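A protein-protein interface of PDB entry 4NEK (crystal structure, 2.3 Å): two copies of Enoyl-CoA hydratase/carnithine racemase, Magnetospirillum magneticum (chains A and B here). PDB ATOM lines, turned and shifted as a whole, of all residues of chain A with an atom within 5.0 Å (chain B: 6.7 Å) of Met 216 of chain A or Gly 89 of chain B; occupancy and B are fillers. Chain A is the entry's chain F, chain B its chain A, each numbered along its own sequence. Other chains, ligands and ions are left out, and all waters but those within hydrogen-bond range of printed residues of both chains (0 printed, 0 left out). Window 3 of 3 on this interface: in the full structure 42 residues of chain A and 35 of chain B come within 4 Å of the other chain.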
ATOM      1  N   PRO A 214      -9.601 -37.909  19.967  1.00  0.00           N
ATOM      2  CA  PRO A 214      -9.783 -36.456  19.955  1.00  0.00           C
ATOM      3  C   PRO A 214      -8.476 -35.754  19.676  1.00  0.00           C
ATOM      4  O   PRO A 214      -7.421 -36.129  20.193  1.00  0.00           O
ATOM      5  CB  PRO A 214     -10.259 -36.145  21.371  1.00  0.00           C
ATOM      6  CG  PRO A 214     -10.959 -37.409  21.797  1.00  0.00           C
ATOM      7  CD  PRO A 214     -10.145 -38.531  21.188  1.00  0.00           C
ATOM      8  N   ILE A 215      -8.552 -34.740  18.832  1.00  0.00           N
ATOM      9  CA  ILE A 215      -7.370 -34.129  18.269  1.00  0.00           C
ATOM     10  C   ILE A 215      -6.398 -33.647  19.336  1.00  0.00           C
ATOM     11  O   ILE A 215      -5.187 -33.843  19.197  1.00  0.00           O
ATOM     12  CB  ILE A 215      -7.762 -33.008  17.275  1.00  0.00           C
ATOM     13  CG1 ILE A 215      -6.583 -32.609  16.417  1.00  0.00           C
ATOM     14  CG2 ILE A 215      -8.329 -31.793  18.001  1.00  0.00           C
ATOM     15  CD1 ILE A 215      -6.047 -33.765  15.588  1.00  0.00           C
ATOM     16  N   MET A 216      -6.891 -33.059  20.424  1.00  0.00           N
ATOM     17  CA  MET A 216      -5.968 -32.570  21.495  1.00  0.00           C
ATOM     18  C   MET A 216      -5.215 -33.701  22.116  1.00  0.00           C
ATOM     19  O   MET A 216      -4.038 -33.569  22.413  1.00  0.00           O
ATOM     20  CB  MET A 216      -6.677 -31.757  22.584  1.00  0.00           C
ATOM     21  CG  MET A 216      -7.450 -30.544  22.041  1.00  0.00           C
ATOM     22  SD  MET A 216      -6.329 -29.176  21.102  1.00  0.00           S
ATOM     23  CE  MET A 216      -7.638 -28.226  19.973  1.00  0.00           C
ATOM     24  N   ASP A 217      -5.857 -34.856  22.294  1.00  0.00           N
ATOM     25  CA  ASP A 217      -5.141 -36.053  22.795  1.00  0.00           C
ATOM     26  C   ASP A 217      -4.051 -36.492  21.864  1.00  0.00           C
ATOM     27  O   ASP A 217      -2.966 -36.839  22.296  1.00  0.00           O
ATOM     28  CB  ASP A 217      -6.081 -37.236  22.979  1.00  0.00           C
ATOM     29  CG  ASP A 217      -7.163 -36.996  24.053  1.00  0.00           C
ATOM     30  OD1 ASP A 217      -7.028 -36.063  24.859  1.00  0.00           O
ATOM     31  OD2 ASP A 217      -8.149 -37.766  24.089  1.00  0.00           O
ATOM     32  N   ARG A 218      -4.319 -36.466  20.568  1.00  0.00           N
ATOM     33  CA  ARG A 218      -3.293 -36.847  19.621  1.00  0.00           C
ATOM     34  C   ARG A 218      -2.108 -35.870  19.656  1.00  0.00           C
ATOM     35  O   ARG A 218      -0.956 -36.272  19.522  1.00  0.00           O
ATOM     36  CB  ARG A 218      -3.867 -36.967  18.186  1.00  0.00           C
ATOM     37  CG  ARG A 218      -2.850 -37.313  17.104  1.00  0.00           C
ATOM     38  CD  ARG A 218      -2.046 -38.576  17.444  1.00  0.00           C
ATOM     39  NE  ARG A 218      -2.943 -39.723  17.482  1.00  0.00           N
ATOM     40  CZ  ARG A 218      -3.061 -40.625  16.519  1.00  0.00           C
ATOM     41  NH1 ARG A 218      -2.281 -40.586  15.445  1.00  0.00           N
ATOM     42  NH2 ARG A 218      -3.956 -41.600  16.647  1.00  0.00           N
ATOM     43  N   LEU A 219      -2.384 -34.584  19.780  1.00  0.00           N
ATOM     44  CA  LEU A 219      -1.304 -33.596  19.843  1.00  0.00           C
ATOM     45  C   LEU A 219      -0.411 -33.886  21.012  1.00  0.00           C
ATOM     46  O   LEU A 219       0.804 -33.829  20.915  1.00  0.00           O
ATOM     47  CB  LEU A 219      -1.865 -32.182  19.980  1.00  0.00           C
ATOM     48  CG  LEU A 219      -2.561 -31.679  18.723  1.00  0.00           C
ATOM     49  CD1 LEU A 219      -3.204 -30.328  18.964  1.00  0.00           C
ATOM     50  CD2 LEU A 219      -1.575 -31.577  17.593  1.00  0.00           C
ATOM     51  N   THR A 220      -1.039 -34.191  22.139  1.00  0.00           N
ATOM     52  CA  THR A 220      -0.310 -34.520  23.343  1.00  0.00           C
ATOM     53  C   THR A 220       0.529 -35.772  23.126  1.00  0.00           C
ATOM     54  O   THR A 220       1.709 -35.819  23.486  1.00  0.00           O
ATOM     55  CB  THR A 220      -1.301 -34.726  24.503  1.00  0.00           C
ATOM     56  OG1 THR A 220      -1.930 -33.483  24.772  1.00  0.00           O
ATOM     57  CG2 THR A 220      -0.619 -35.176  25.737  1.00  0.00           C
ATOM     58  N   GLU B  43     -10.514 -15.023  18.433  1.00  0.00           N
ATOM     59  CA  GLU B  43     -11.513 -15.933  18.982  1.00  0.00           C
ATOM     60  C   GLU B  43     -12.438 -15.249  19.941  1.00  0.00           C
ATOM     61  O   GLU B  43     -13.605 -15.563  19.972  1.00  0.00           O
ATOM     62  CB  GLU B  43     -10.858 -17.122  19.668  1.00  0.00           C
ATOM     63  CG  GLU B  43     -10.411 -18.188  18.682  1.00  0.00           C
ATOM     64  CD  GLU B  43     -11.576 -19.067  18.223  1.00  0.00           C
ATOM     65  OE1 GLU B  43     -12.046 -19.918  19.019  1.00  0.00           O
ATOM     66  OE2 GLU B  43     -12.008 -18.912  17.060  1.00  0.00           O
ATOM     67  N   ILE B  84      -0.200 -24.158  17.594  1.00  0.00           N
ATOM     68  CA  ILE B  84      -0.895 -25.283  17.028  1.00  0.00           C
ATOM     69  C   ILE B  84      -2.233 -25.526  17.727  1.00  0.00           C
ATOM     70  O   ILE B  84      -3.275 -25.717  17.085  1.00  0.00           O
ATOM     71  CB  ILE B  84      -0.020 -26.559  17.116  1.00  0.00           C
ATOM     72  CG1 ILE B  84       1.230 -26.423  16.225  1.00  0.00           C
ATOM     73  CG2 ILE B  84      -0.811 -27.776  16.677  1.00  0.00           C
ATOM     74  CD1 ILE B  84       2.409 -27.312  16.638  1.00  0.00           C
ATOM     75  N   ARG B  85      -2.216 -25.536  19.047  1.00  0.00           N
ATOM     76  CA  ARG B  85      -3.470 -25.763  19.774  1.00  0.00           C
ATOM     77  C   ARG B  85      -4.449 -24.676  19.476  1.00  0.00           C
ATOM     78  O   ARG B  85      -5.646 -24.939  19.390  1.00  0.00           O
ATOM     79  CB  ARG B  85      -3.229 -25.939  21.268  1.00  0.00           C
ATOM     80  CG  ARG B  85      -2.536 -27.278  21.522  1.00  0.00           C
ATOM     81  CD  ARG B  85      -2.168 -27.506  22.956  1.00  0.00           C
ATOM     82  NE  ARG B  85      -1.459 -28.777  23.067  1.00  0.00           N
ATOM     83  CZ  ARG B  85      -2.019 -29.947  23.359  1.00  0.00           C
ATOM     84  NH1 ARG B  85      -3.318 -30.044  23.600  1.00  0.00           N
ATOM     85  NH2 ARG B  85      -1.261 -31.041  23.432  1.00  0.00           N
ATOM     86  N   ALA B  86      -3.946 -23.459  19.358  1.00  0.00           N
ATOM     87  CA  ALA B  86      -4.835 -22.336  19.136  1.00  0.00           C
ATOM     88  C   ALA B  86      -5.585 -22.502  17.835  1.00  0.00           C
ATOM     89  O   ALA B  86      -6.775 -22.238  17.774  1.00  0.00           O
ATOM     90  CB  ALA B  86      -4.084 -21.050  19.139  1.00  0.00           C
ATOM     91  N   VAL B  87      -4.919 -23.010  16.823  1.00  0.00           N
ATOM     92  CA  VAL B  87      -5.595 -23.241  15.558  1.00  0.00           C
ATOM     93  C   VAL B  87      -6.479 -24.479  15.556  1.00  0.00           C
ATOM     94  O   VAL B  87      -7.595 -24.451  15.085  1.00  0.00           O
ATOM     95  CB  VAL B  87      -4.580 -23.356  14.415  1.00  0.00           C
ATOM     96  CG1 VAL B  87      -5.316 -23.599  13.110  1.00  0.00           C
ATOM     97  CG2 VAL B  87      -3.760 -22.074  14.322  1.00  0.00           C
ATOM     98  N   ALA B  88      -5.950 -25.587  16.040  1.00  0.00           N
ATOM     99  CA  ALA B  88      -6.710 -26.811  16.114  1.00  0.00           C
ATOM    100  C   ALA B  88      -7.965 -26.634  16.899  1.00  0.00           C
ATOM    101  O   ALA B  88      -8.997 -27.204  16.547  1.00  0.00           O
ATOM    102  CB  ALA B  88      -5.871 -27.878  16.754  1.00  0.00           C
ATOM    103  N   GLY B  89      -7.905 -25.830  17.965  1.00  0.00           N
ATOM    104  CA  GLY B  89      -9.077 -25.573  18.808  1.00  0.00           C
ATOM    105  C   GLY B  89      -9.907 -24.343  18.432  1.00  0.00           C
ATOM    106  O   GLY B  89     -10.926 -24.063  19.088  1.00  0.00           O
ATOM    107  N   ALA B  90      -9.551 -23.647  17.356  1.00  0.00           N
ATOM    108  CA  ALA B  90     -10.318 -22.457  17.002  1.00  0.00           C
ATOM    109  C   ALA B  90     -11.759 -22.792  16.643  1.00  0.00           C
ATOM    110  O   ALA B  90     -12.010 -23.649  15.801  1.00  0.00           O
ATOM    111  CB  ALA B  90      -9.672 -21.722  15.858  1.00  0.00           C
ATOM    112  N   ARG B  91     -12.698 -22.098  17.286  1.00  0.00           N
ATOM    113  CA  ARG B  91     -14.114 -22.298  17.071  1.00  0.00           C
ATOM    114  C   ARG B  91     -14.556 -21.621  15.789  1.00  0.00           C
ATOM    115  O   ARG B  91     -15.441 -22.121  15.096  1.00  0.00           O
ATOM    116  CB  ARG B  91     -14.887 -21.779  18.274  1.00  0.00           C
ATOM    117  CG  ARG B  91     -14.570 -22.522  19.584  1.00  0.00           C
ATOM    118  CD  ARG B  91     -15.422 -23.787  19.834  1.00  0.00           C
ATOM    119  NE  ARG B  91     -16.891 -23.558  19.794  1.00  0.00           N
ATOM    120  CZ  ARG B  91     -17.838 -24.443  20.138  1.00  0.00           C
ATOM    121  NH1 ARG B  91     -17.522 -25.650  20.583  1.00  0.00           N
ATOM    122  NH2 ARG B  91     -19.134 -24.120  20.028  1.00  0.00           N
ATOM    123  N   LYS B  92     -13.913 -20.512  15.426  1.00  0.00           N
ATOM    124  CA  LYS B  92     -14.263 -19.821  14.201  1.00  0.00           C
ATOM    125  C   LYS B  92     -13.541 -20.413  12.994  1.00  0.00           C
ATOM    126  O   LYS B  92     -12.499 -21.041  13.140  1.00  0.00           O
ATOM    127  CB  LYS B  92     -13.963 -18.322  14.307  1.00  0.00           C
ATOM    128  CG  LYS B  92     -14.708 -17.668  15.441  1.00  0.00           C
ATOM    129  CD  LYS B  92     -14.402 -16.184  15.611  1.00  0.00           C
ATOM    130  CE  LYS B  92     -15.130 -15.653  16.845  1.00  0.00           C
ATOM    131  NZ  LYS B  92     -14.853 -14.219  17.090  1.00  0.00           N
ATOM    132  N   HIS B 112      -6.086 -28.484   9.905  1.00  0.00           N
ATOM    133  CA  HIS B 112      -6.925 -27.782  10.837  1.00  0.00           C
ATOM    134  C   HIS B 112      -7.652 -26.606  10.201  1.00  0.00           C
ATOM    135  O   HIS B 112      -8.428 -25.978  10.870  1.00  0.00           O
ATOM    136  CB  HIS B 112      -6.069 -27.300  11.996  1.00  0.00           C
ATOM    137  CG  HIS B 112      -5.302 -28.407  12.617  1.00  0.00           C
ATOM    138  ND1 HIS B 112      -5.920 -29.440  13.280  1.00  0.00           N
ATOM    139  CD2 HIS B 112      -3.985 -28.712  12.576  1.00  0.00           C
ATOM    140  CE1 HIS B 112      -5.008 -30.294  13.694  1.00  0.00           C
ATOM    141  NE2 HIS B 112      -3.824 -29.874  13.284  1.00  0.00           N
ATOM    142  N   LYS B 205     -19.188 -26.196  12.329  1.00  0.00           N
ATOM    143  CA  LYS B 205     -17.804 -26.550  12.390  1.00  0.00           C
ATOM    144  C   LYS B 205     -17.571 -27.488  13.562  1.00  0.00           C
ATOM    145  O   LYS B 205     -16.857 -28.483  13.432  1.00  0.00           O
ATOM    146  CB  LYS B 205     -16.921 -25.308  12.497  1.00  0.00           C
ATOM    147  CG  LYS B 205     -15.475 -25.654  12.703  1.00  0.00           C
ATOM    148  CD  LYS B 205     -14.586 -24.456  12.494  1.00  0.00           C
ATOM    149  CE  LYS B 205     -13.202 -24.814  12.968  1.00  0.00           C
ATOM    150  NZ  LYS B 205     -12.170 -23.807  12.635  1.00  0.00           N
ATOM    151  N   LYS B 209     -16.204 -31.375  13.416  1.00  0.00           N
ATOM    152  CA  LYS B 209     -14.947 -31.735  14.063  1.00  0.00           C
ATOM    153  C   LYS B 209     -15.131 -32.580  15.309  1.00  0.00           C
ATOM    154  O   LYS B 209     -14.167 -32.908  15.956  1.00  0.00           O
ATOM    155  CB  LYS B 209     -14.161 -30.477  14.381  1.00  0.00           C
ATOM    156  CG  LYS B 209     -13.737 -29.809  13.080  1.00  0.00           C
ATOM    157  CD  LYS B 209     -12.878 -28.584  13.276  1.00  0.00           C
ATOM    158  CE  LYS B 209     -11.526 -28.934  13.844  1.00  0.00           C
ATOM    159  NZ  LYS B 209     -10.601 -27.783  13.734  1.00  0.00           N
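The guanidinium group of Arg 85 of chain B lies within hydrogen-bond range of the side-chain hydroxyl of Thr 220 of chain A, at 2.9 Å.
O of Met 216 of chain A lies within hydrogen-bond range of OG1 of Thr 220 of chain A. The side-chain amino group (NZ) of Lys 209 of chain B sits at hydrogen-bond distance from the backbone carbonyl oxygen (O) of Ala 88 of chain B (3.3 Å).
Among the printed residues, merely in contact across the chains: Ile 215 of chain A with His 112 of chain B, Met 216 of chain A with Arg 85 of chain B, Met 216 of chain A with Ala 88 of chain B, Met 216 of chain A with Gly 89 of chain B, Leu 219 of chain A with Ile 84 of chain B and Leu 219 of chain A with Arg 85 of chain B.
Of chain A, only Met 216 comes within 4 Å of Gly 89 of chain B. Of the printed residues of chain A, Ala 88 of chain B touches Met 216 (3.5 Å). Of the printed residues of chain B, Thr 220 of chain A touches Arg 85. Of the printed residues of chain A, Arg 85 of chain B touches Met 216, Leu 219 and Thr 220. Of the printed residues of chain A, Ile 84 of chain B touches Leu 219 (3.98 Å). Of the printed residues of chain B, Ile 215 of chain A touches His 112 (3.9 Å).
Of the 13 printed residues of chain B, 5 touch a printed residue of chain A. Printed residues of chain B that touch a printed residue of chain A: Ile 84, Arg 85, Ala 88, Gly 89 and His 112. Among the printed residues, 7 pairs touch across the chains. Among the printed residues, no Asp or Glu carboxylate lies within 4 Å of a Lys or Arg side-chain nitrogen of the other chain.
No position is printed for both chains.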
